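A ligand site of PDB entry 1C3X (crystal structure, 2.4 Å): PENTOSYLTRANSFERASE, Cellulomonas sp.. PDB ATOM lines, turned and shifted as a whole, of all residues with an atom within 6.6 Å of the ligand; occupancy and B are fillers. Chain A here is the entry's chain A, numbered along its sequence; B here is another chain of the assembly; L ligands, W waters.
The backbone carbonyl oxygen (O) of Gly 119 lies within hydrogen-bond range of a nitrogen (N1) of the ligand.
OE2 of Glu 188 lies within hydrogen-bond range of N2 of the ligand.
The backbone NH of Thr 229 lies within hydrogen-bond range of the backbone carbonyl oxygen of Cys 120 (2.7 Å).
The backbone carbonyl oxygen (O) of Val 204 sits at hydrogen-bond distance from the backbone NH (N) of Gly 121.
The side-chain hydroxyl (OH) of Tyr 179 sits at hydrogen-bond distance from the backbone NH (N) of Met 206.
The backbone carbonyl oxygen (O) of Ser 38 sits close to the backbone NH (N) of Gly 119 (3.4 Å).
The backbone carbonyl oxygen (O) of Gly 205 lies within hydrogen-bond range of the backbone NH (N) of Phe 182, 2.9 Å away.
The backbone NH of Gly 205 sits at hydrogen-bond distance from the backbone carbonyl oxygen of Ala 180.
The backbone carbonyl oxygen (O) of Leu 227 lies within hydrogen-bond range of the backbone NH (N) of Cys 120 (3.2 Å).
Residues that only touch the ligand: Thr 229 (2.7 Å), Met 206 (3.2 Å), Gly 121 (3.4 Å), Tyr 187 (3.4 Å), Gly 205 (3.5 Å), Cys 120 (3.5 Å) and Val 204 (3.6 Å).
Hydrophobic or aromatic side chains within 4 Å of the ligand: Tyr 187, Val 204 and Met 206.
Of the 28 residues printed, 9 come within 4 Å of the ligand.
The nearest printed residue that does not touch the ligand is Ser 38 (4.2 Å).
Water W1 bridges an oxygen (O1) of the ligand (2.8 Å) and the side-chain amide nitrogen (ND2) of Asn 230 (3.0 Å).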
ATOM      1  N   SER A  38     -26.596 -30.440 -29.525  1.00  0.00           N
ATOM      2  CA  SER A  38     -25.448 -30.508 -30.402  1.00  0.00           C
ATOM      3  C   SER A  38     -24.453 -31.470 -29.788  1.00  0.00           C
ATOM      4  O   SER A  38     -24.018 -31.263 -28.644  1.00  0.00           O
ATOM      5  CB  SER A  38     -24.820 -29.134 -30.579  1.00  0.00           C
ATOM      6  OG  SER A  38     -25.104 -28.660 -31.889  1.00  0.00           O
ATOM      7  N   GLY A  39     -24.101 -32.496 -30.586  1.00  0.00           N
ATOM      8  CA  GLY A  39     -23.198 -33.544 -30.155  1.00  0.00           C
ATOM      9  C   GLY A  39     -23.934 -34.782 -29.619  1.00  0.00           C
ATOM     10  O   GLY A  39     -23.290 -35.790 -29.290  1.00  0.00           O
ATOM     11  N   ASN A 118     -27.252 -30.773 -24.259  1.00  0.00           N
ATOM     12  CA  ASN A 118     -26.880 -29.717 -25.208  1.00  0.00           C
ATOM     13  C   ASN A 118     -25.363 -29.646 -25.307  1.00  0.00           C
ATOM     14  O   ASN A 118     -24.640 -30.254 -24.491  1.00  0.00           O
ATOM     15  CB  ASN A 118     -27.386 -28.350 -24.737  1.00  0.00           C
ATOM     16  CG  ASN A 118     -26.655 -27.876 -23.515  1.00  0.00           C
ATOM     17  OD1 ASN A 118     -27.248 -27.630 -22.456  1.00  0.00           O
ATOM     18  ND2 ASN A 118     -25.327 -27.774 -23.634  1.00  0.00           N
ATOM     19  N   GLY A 119     -24.885 -28.917 -26.300  1.00  0.00           N
ATOM     20  CA  GLY A 119     -23.456 -28.722 -26.464  1.00  0.00           C
ATOM     21  C   GLY A 119     -23.182 -27.282 -26.025  1.00  0.00           C
ATOM     22  O   GLY A 119     -23.987 -26.379 -26.314  1.00  0.00           O
ATOM     23  N   CYS A 120     -22.055 -27.040 -25.362  1.00  0.00           N
ATOM     24  CA  CYS A 120     -21.818 -25.688 -24.898  1.00  0.00           C
ATOM     25  C   CYS A 120     -20.342 -25.454 -24.803  1.00  0.00           C
ATOM     26  O   CYS A 120     -19.552 -26.337 -25.160  1.00  0.00           O
ATOM     27  CB  CYS A 120     -22.440 -25.528 -23.519  1.00  0.00           C
ATOM     28  SG  CYS A 120     -21.687 -26.689 -22.429  1.00  0.00           S
ATOM     29  N   GLY A 121     -19.979 -24.233 -24.371  1.00  0.00           N
ATOM     30  CA  GLY A 121     -18.583 -23.877 -24.157  1.00  0.00           C
ATOM     31  C   GLY A 121     -18.359 -24.053 -22.650  1.00  0.00           C
ATOM     32  O   GLY A 121     -19.289 -23.811 -21.850  1.00  0.00           O
ATOM     33  N   GLY A 122     -17.164 -24.512 -22.261  1.00  0.00           N
ATOM     34  CA  GLY A 122     -16.885 -24.688 -20.851  1.00  0.00           C
ATOM     35  C   GLY A 122     -15.949 -23.591 -20.342  1.00  0.00           C
ATOM     36  O   GLY A 122     -15.165 -23.032 -21.118  1.00  0.00           O
ATOM     37  N   TYR A 179     -25.229 -23.828 -15.646  1.00  0.00           N
ATOM     38  CA  TYR A 179     -25.324 -23.476 -17.073  1.00  0.00           C
ATOM     39  C   TYR A 179     -25.985 -22.118 -17.344  1.00  0.00           C
ATOM     40  O   TYR A 179     -27.064 -21.809 -16.797  1.00  0.00           O
ATOM     41  CB  TYR A 179     -26.108 -24.591 -17.770  1.00  0.00           C
ATOM     42  CG  TYR A 179     -26.425 -24.376 -19.223  1.00  0.00           C
ATOM     43  CD1 TYR A 179     -27.372 -23.450 -19.619  1.00  0.00           C
ATOM     44  CD2 TYR A 179     -25.771 -25.097 -20.213  1.00  0.00           C
ATOM     45  CE1 TYR A 179     -27.658 -23.236 -20.991  1.00  0.00           C
ATOM     46  CE2 TYR A 179     -26.036 -24.902 -21.552  1.00  0.00           C
ATOM     47  CZ  TYR A 179     -26.978 -23.964 -21.944  1.00  0.00           C
ATOM     48  OH  TYR A 179     -27.209 -23.724 -23.293  1.00  0.00           O
ATOM     49  N   ALA A 180     -25.370 -21.332 -18.250  1.00  0.00           N
ATOM     50  CA  ALA A 180     -25.899 -20.021 -18.574  1.00  0.00           C
ATOM     51  C   ALA A 180     -26.427 -19.997 -19.981  1.00  0.00           C
ATOM     52  O   ALA A 180     -25.718 -20.332 -20.921  1.00  0.00           O
ATOM     53  CB  ALA A 180     -24.789 -18.916 -18.410  1.00  0.00           C
ATOM     54  N   GLN A 181     -27.687 -19.617 -20.171  1.00  0.00           N
ATOM     55  CA  GLN A 181     -28.174 -19.539 -21.529  1.00  0.00           C
ATOM     56  C   GLN A 181     -28.130 -18.109 -22.072  1.00  0.00           C
ATOM     57  O   GLN A 181     -28.738 -17.195 -21.483  1.00  0.00           O
ATOM     58  CB  GLN A 181     -29.613 -20.045 -21.599  1.00  0.00           C
ATOM     59  CG  GLN A 181     -30.231 -19.921 -23.003  1.00  0.00           C
ATOM     60  CD  GLN A 181     -31.672 -20.471 -23.134  1.00  0.00           C
ATOM     61  OE1 GLN A 181     -32.264 -20.408 -24.240  1.00  0.00           O
ATOM     62  NE2 GLN A 181     -32.242 -20.999 -22.045  1.00  0.00           N
ATOM     63  N   PHE A 182     -27.398 -17.889 -23.141  1.00  0.00           N
ATOM     64  CA  PHE A 182     -27.357 -16.594 -23.781  1.00  0.00           C
ATOM     65  C   PHE A 182     -28.318 -16.806 -24.966  1.00  0.00           C
ATOM     66  O   PHE A 182     -28.617 -17.951 -25.345  1.00  0.00           O
ATOM     67  CB  PHE A 182     -25.946 -16.280 -24.354  1.00  0.00           C
ATOM     68  CG  PHE A 182     -24.939 -15.830 -23.343  1.00  0.00           C
ATOM     69  CD1 PHE A 182     -24.508 -16.695 -22.349  1.00  0.00           C
ATOM     70  CD2 PHE A 182     -24.437 -14.520 -23.359  1.00  0.00           C
ATOM     71  CE1 PHE A 182     -23.594 -16.258 -21.372  1.00  0.00           C
ATOM     72  CE2 PHE A 182     -23.515 -14.075 -22.391  1.00  0.00           C
ATOM     73  CZ  PHE A 182     -23.101 -14.952 -21.388  1.00  0.00           C
ATOM     74  N   GLY A 184     -27.825 -15.980 -28.142  1.00  0.00           N
ATOM     75  CA  GLY A 184     -27.092 -16.288 -29.361  1.00  0.00           C
ATOM     76  C   GLY A 184     -27.726 -15.650 -30.575  1.00  0.00           C
ATOM     77  O   GLY A 184     -28.486 -14.685 -30.430  1.00  0.00           O
ATOM     78  N   PRO A 185     -27.448 -16.145 -31.788  1.00  0.00           N
ATOM     79  CA  PRO A 185     -26.570 -17.268 -32.139  1.00  0.00           C
ATOM     80  C   PRO A 185     -25.054 -16.954 -32.095  1.00  0.00           C
ATOM     81  O   PRO A 185     -24.243 -17.890 -32.127  1.00  0.00           O
ATOM     82  CB  PRO A 185     -27.049 -17.665 -33.527  1.00  0.00           C
ATOM     83  CG  PRO A 185     -27.326 -16.302 -34.138  1.00  0.00           C
ATOM     84  CD  PRO A 185     -28.117 -15.621 -32.999  1.00  0.00           C
ATOM     85  N   HIS A 186     -24.636 -15.678 -32.022  1.00  0.00           N
ATOM     86  CA  HIS A 186     -23.207 -15.392 -31.952  1.00  0.00           C
ATOM     87  C   HIS A 186     -22.649 -16.009 -30.683  1.00  0.00           C
ATOM     88  O   HIS A 186     -23.414 -16.370 -29.775  1.00  0.00           O
ATOM     89  CB  HIS A 186     -22.883 -13.883 -31.976  1.00  0.00           C
ATOM     90  CG  HIS A 186     -23.636 -13.069 -30.975  1.00  0.00           C
ATOM     91  ND1 HIS A 186     -24.915 -12.572 -31.224  1.00  0.00           N
ATOM     92  CD2 HIS A 186     -23.376 -12.791 -29.672  1.00  0.00           C
ATOM     93  CE1 HIS A 186     -25.389 -12.033 -30.111  1.00  0.00           C
ATOM     94  NE2 HIS A 186     -24.475 -12.149 -29.161  1.00  0.00           N
ATOM     95  N   TYR A 187     -21.330 -16.203 -30.647  1.00  0.00           N
ATOM     96  CA  TYR A 187     -20.705 -16.774 -29.480  1.00  0.00           C
ATOM     97  C   TYR A 187     -20.319 -15.609 -28.594  1.00  0.00           C
ATOM     98  O   TYR A 187     -20.363 -14.470 -29.020  1.00  0.00           O
ATOM     99  CB  TYR A 187     -19.467 -17.577 -29.852  1.00  0.00           C
ATOM    100  CG  TYR A 187     -19.809 -18.914 -30.444  1.00  0.00           C
ATOM    101  CD1 TYR A 187     -20.709 -19.749 -29.803  1.00  0.00           C
ATOM    102  CD2 TYR A 187     -19.231 -19.345 -31.630  1.00  0.00           C
ATOM    103  CE1 TYR A 187     -21.035 -21.001 -30.331  1.00  0.00           C
ATOM    104  CE2 TYR A 187     -19.555 -20.602 -32.171  1.00  0.00           C
ATOM    105  CZ  TYR A 187     -20.462 -21.419 -31.500  1.00  0.00           C
ATOM    106  OH  TYR A 187     -20.809 -22.651 -32.016  1.00  0.00           O
ATOM    107  N   GLU A 188     -19.898 -15.902 -27.377  1.00  0.00           N
ATOM    108  CA  GLU A 188     -19.521 -14.862 -26.463  1.00  0.00           C
ATOM    109  C   GLU A 188     -18.117 -14.347 -26.689  1.00  0.00           C
ATOM    110  O   GLU A 188     -17.259 -15.063 -27.177  1.00  0.00           O
ATOM    111  CB  GLU A 188     -19.599 -15.365 -25.013  1.00  0.00           C
ATOM    112  CG  GLU A 188     -20.981 -15.862 -24.531  1.00  0.00           C
ATOM    113  CD  GLU A 188     -21.483 -17.037 -25.335  1.00  0.00           C
ATOM    114  OE1 GLU A 188     -20.723 -18.027 -25.501  1.00  0.00           O
ATOM    115  OE2 GLU A 188     -22.657 -16.964 -25.775  1.00  0.00           O
ATOM    116  N   VAL A 193     -17.472 -13.915 -21.716  1.00  0.00           N
ATOM    117  CA  VAL A 193     -17.206 -15.231 -21.063  1.00  0.00           C
ATOM    118  C   VAL A 193     -16.773 -15.070 -19.630  1.00  0.00           C
ATOM    119  O   VAL A 193     -17.217 -15.823 -18.752  1.00  0.00           O
ATOM    120  CB  VAL A 193     -16.123 -16.051 -21.818  1.00  0.00           C
ATOM    121  CG1 VAL A 193     -15.662 -17.268 -20.962  1.00  0.00           C
ATOM    122  CG2 VAL A 193     -16.728 -16.535 -23.122  1.00  0.00           C
ATOM    123  N   VAL A 204     -21.682 -22.219 -20.853  1.00  0.00           N
ATOM    124  CA  VAL A 204     -22.491 -21.252 -21.596  1.00  0.00           C
ATOM    125  C   VAL A 204     -22.998 -21.953 -22.808  1.00  0.00           C
ATOM    126  O   VAL A 204     -22.275 -22.732 -23.418  1.00  0.00           O
ATOM    127  CB  VAL A 204     -21.676 -20.066 -22.101  1.00  0.00           C
ATOM    128  CG1 VAL A 204     -21.201 -19.199 -20.914  1.00  0.00           C
ATOM    129  CG2 VAL A 204     -20.522 -20.584 -22.911  1.00  0.00           C
ATOM    130  N   GLY A 205     -24.253 -21.676 -23.151  1.00  0.00           N
ATOM    131  CA  GLY A 205     -24.870 -22.306 -24.315  1.00  0.00           C
ATOM    132  C   GLY A 205     -26.029 -21.445 -24.754  1.00  0.00           C
ATOM    133  O   GLY A 205     -26.234 -20.377 -24.174  1.00  0.00           O
ATOM    134  N   MET A 206     -26.797 -21.889 -25.750  1.00  0.00           N
ATOM    135  CA  MET A 206     -27.940 -21.133 -26.278  1.00  0.00           C
ATOM    136  C   MET A 206     -29.296 -21.824 -26.164  1.00  0.00           C
ATOM    137  O   MET A 206     -30.201 -21.609 -26.988  1.00  0.00           O
ATOM    138  CB  MET A 206     -27.716 -20.830 -27.748  1.00  0.00           C
ATOM    139  CG  MET A 206     -26.343 -20.268 -28.027  1.00  0.00           C
ATOM    140  SD  MET A 206     -26.151 -20.033 -29.781  1.00  0.00           S
ATOM    141  CE  MET A 206     -24.389 -20.015 -29.836  1.00  0.00           C
ATOM    142  N   SER A 207     -29.501 -22.622 -25.118  1.00  0.00           N
ATOM    143  CA  SER A 207     -30.786 -23.276 -25.013  1.00  0.00           C
ATOM    144  C   SER A 207     -31.021 -23.844 -23.626  1.00  0.00           C
ATOM    145  O   SER A 207     -30.444 -23.413 -22.635  1.00  0.00           O
ATOM    146  CB  SER A 207     -30.805 -24.423 -26.034  1.00  0.00           C
ATOM    147  OG  SER A 207     -29.811 -25.379 -25.680  1.00  0.00           O
ATOM    148  N   LEU A 227     -22.551 -31.246 -22.935  1.00  0.00           N
ATOM    149  CA  LEU A 227     -21.367 -31.882 -23.525  1.00  0.00           C
ATOM    150  C   LEU A 227     -20.485 -30.699 -23.934  1.00  0.00           C
ATOM    151  O   LEU A 227     -20.788 -29.996 -24.896  1.00  0.00           O
ATOM    152  CB  LEU A 227     -21.696 -32.658 -24.811  1.00  0.00           C
ATOM    153  CG  LEU A 227     -20.708 -33.780 -25.257  1.00  0.00           C
ATOM    154  CD1 LEU A 227     -20.606 -33.762 -26.777  1.00  0.00           C
ATOM    155  CD2 LEU A 227     -19.315 -33.640 -24.627  1.00  0.00           C
ATOM    156  N   THR A 229     -18.390 -28.706 -25.849  1.00  0.00           N
ATOM    157  CA  THR A 229     -17.910 -28.749 -27.232  1.00  0.00           C
ATOM    158  C   THR A 229     -16.467 -28.274 -27.241  1.00  0.00           C
ATOM    159  O   THR A 229     -15.634 -28.835 -27.945  1.00  0.00           O
ATOM    160  CB  THR A 229     -18.661 -27.786 -28.085  1.00  0.00           C
ATOM    161  OG1 THR A 229     -20.084 -28.043 -27.936  1.00  0.00           O
ATOM    162  CG2 THR A 229     -18.243 -27.956 -29.563  1.00  0.00           C
ATOM    163  N   ASN A 230     -16.162 -27.220 -26.473  1.00  0.00           N
ATOM    164  CA  ASN A 230     -14.786 -26.718 -26.404  1.00  0.00           C
ATOM    165  C   ASN A 230     -14.729 -25.559 -25.418  1.00  0.00           C
ATOM    166  O   ASN A 230     -15.755 -24.953 -25.087  1.00  0.00           O
ATOM    167  CB  ASN A 230     -14.248 -26.452 -27.847  1.00  0.00           C
ATOM    168  CG  ASN A 230     -13.993 -24.982 -28.202  1.00  0.00           C
ATOM    169  OD1 ASN A 230     -12.906 -24.454 -27.963  1.00  0.00           O
ATOM    170  ND2 ASN A 230     -14.994 -24.343 -28.826  1.00  0.00           N
ATOM    171  N   LEU A 231     -13.546 -25.318 -24.874  1.00  0.00           N
ATOM    172  CA  LEU A 231     -13.434 -24.277 -23.891  1.00  0.00           C
ATOM    173  C   LEU A 231     -13.913 -22.975 -24.469  1.00  0.00           C
ATOM    174  O   LEU A 231     -13.656 -22.701 -25.650  1.00  0.00           O
ATOM    175  CB  LEU A 231     -11.984 -24.185 -23.455  1.00  0.00           C
ATOM    176  CG  LEU A 231     -11.518 -25.462 -22.744  1.00  0.00           C
ATOM    177  CD1 LEU A 231     -10.035 -25.299 -22.274  1.00  0.00           C
ATOM    178  CD2 LEU A 231     -12.438 -25.752 -21.561  1.00  0.00           C
ATOM    179  N   ALA A 232     -14.643 -22.160 -23.668  1.00  0.00           N
ATOM    180  CA  ALA A 232     -15.146 -20.855 -24.153  1.00  0.00           C
ATOM    181  C   ALA A 232     -14.022 -19.915 -24.649  1.00  0.00           C
ATOM    182  O   ALA A 232     -12.832 -20.094 -24.321  1.00  0.00           O
ATOM    183  CB  ALA A 232     -16.000 -20.134 -23.030  1.00  0.00           C
ATOM    184  N   ALA A 233     -14.378 -18.880 -25.402  1.00  0.00           N
ATOM    185  CA  ALA A 233     -13.327 -17.970 -25.908  1.00  0.00           C
ATOM    186  C   ALA A 233     -12.480 -17.389 -24.772  1.00  0.00           C
ATOM    187  O   ALA A 233     -12.968 -17.084 -23.686  1.00  0.00           O
ATOM    188  CB  ALA A 233     -13.979 -16.839 -26.765  1.00  0.00           C
ATOM    189  N   PHE B 152     -23.370 -19.277 -36.380  1.00  0.00           N
ATOM    190  CA  PHE B 152     -22.383 -19.314 -35.302  1.00  0.00           C
ATOM    191  C   PHE B 152     -21.058 -18.623 -35.618  1.00  0.00           C
ATOM    192  O   PHE B 152     -20.063 -19.254 -36.051  1.00  0.00           O
ATOM    193  CB  PHE B 152     -22.166 -20.759 -34.900  1.00  0.00           C
ATOM    194  CG  PHE B 152     -23.457 -21.499 -34.697  1.00  0.00           C
ATOM    195  CD1 PHE B 152     -24.487 -20.916 -33.927  1.00  0.00           C
ATOM    196  CD2 PHE B 152     -23.660 -22.757 -35.271  1.00  0.00           C
ATOM    197  CE1 PHE B 152     -25.699 -21.587 -33.743  1.00  0.00           C
ATOM    198  CE2 PHE B 152     -24.868 -23.436 -35.091  1.00  0.00           C
ATOM    199  CZ  PHE B 152     -25.898 -22.853 -34.321  1.00  0.00           C
HETATM  200  I1  LIG L   1     -21.714 -26.467 -29.467  1.00  0.00           I
HETATM  201  O1  LIG L   1     -19.247 -21.491 -26.439  1.00  0.00           O
HETATM  202  C1  LIG L   1     -21.802 -24.579 -28.487  1.00  0.00           C
HETATM  203  N1  LIG L   1     -22.962 -23.846 -28.366  1.00  0.00           N
HETATM  204  N2  LIG L   1     -23.492 -19.583 -26.352  1.00  0.00           N
HETATM  205  N3  LIG L   1     -21.380 -20.597 -26.429  1.00  0.00           N
HETATM  206  C2  LIG L   1     -22.767 -20.660 -26.744  1.00  0.00           C
HETATM  207  N4  LIG L   1     -23.389 -21.718 -27.381  1.00  0.00           N
HETATM  208  C3  LIG L   1     -22.517 -22.735 -27.708  1.00  0.00           C
HETATM  209  C4  LIG L   1     -21.163 -22.815 -27.479  1.00  0.00           C
HETATM  210  C5  LIG L   1     -20.500 -21.655 -26.764  1.00  0.00           C
HETATM  211  N5  LIG L   1     -20.705 -24.004 -27.989  1.00  0.00           N
HETATM  212  O   HOH W   1     -16.882 -22.195 -27.824  1.00  0.00           O
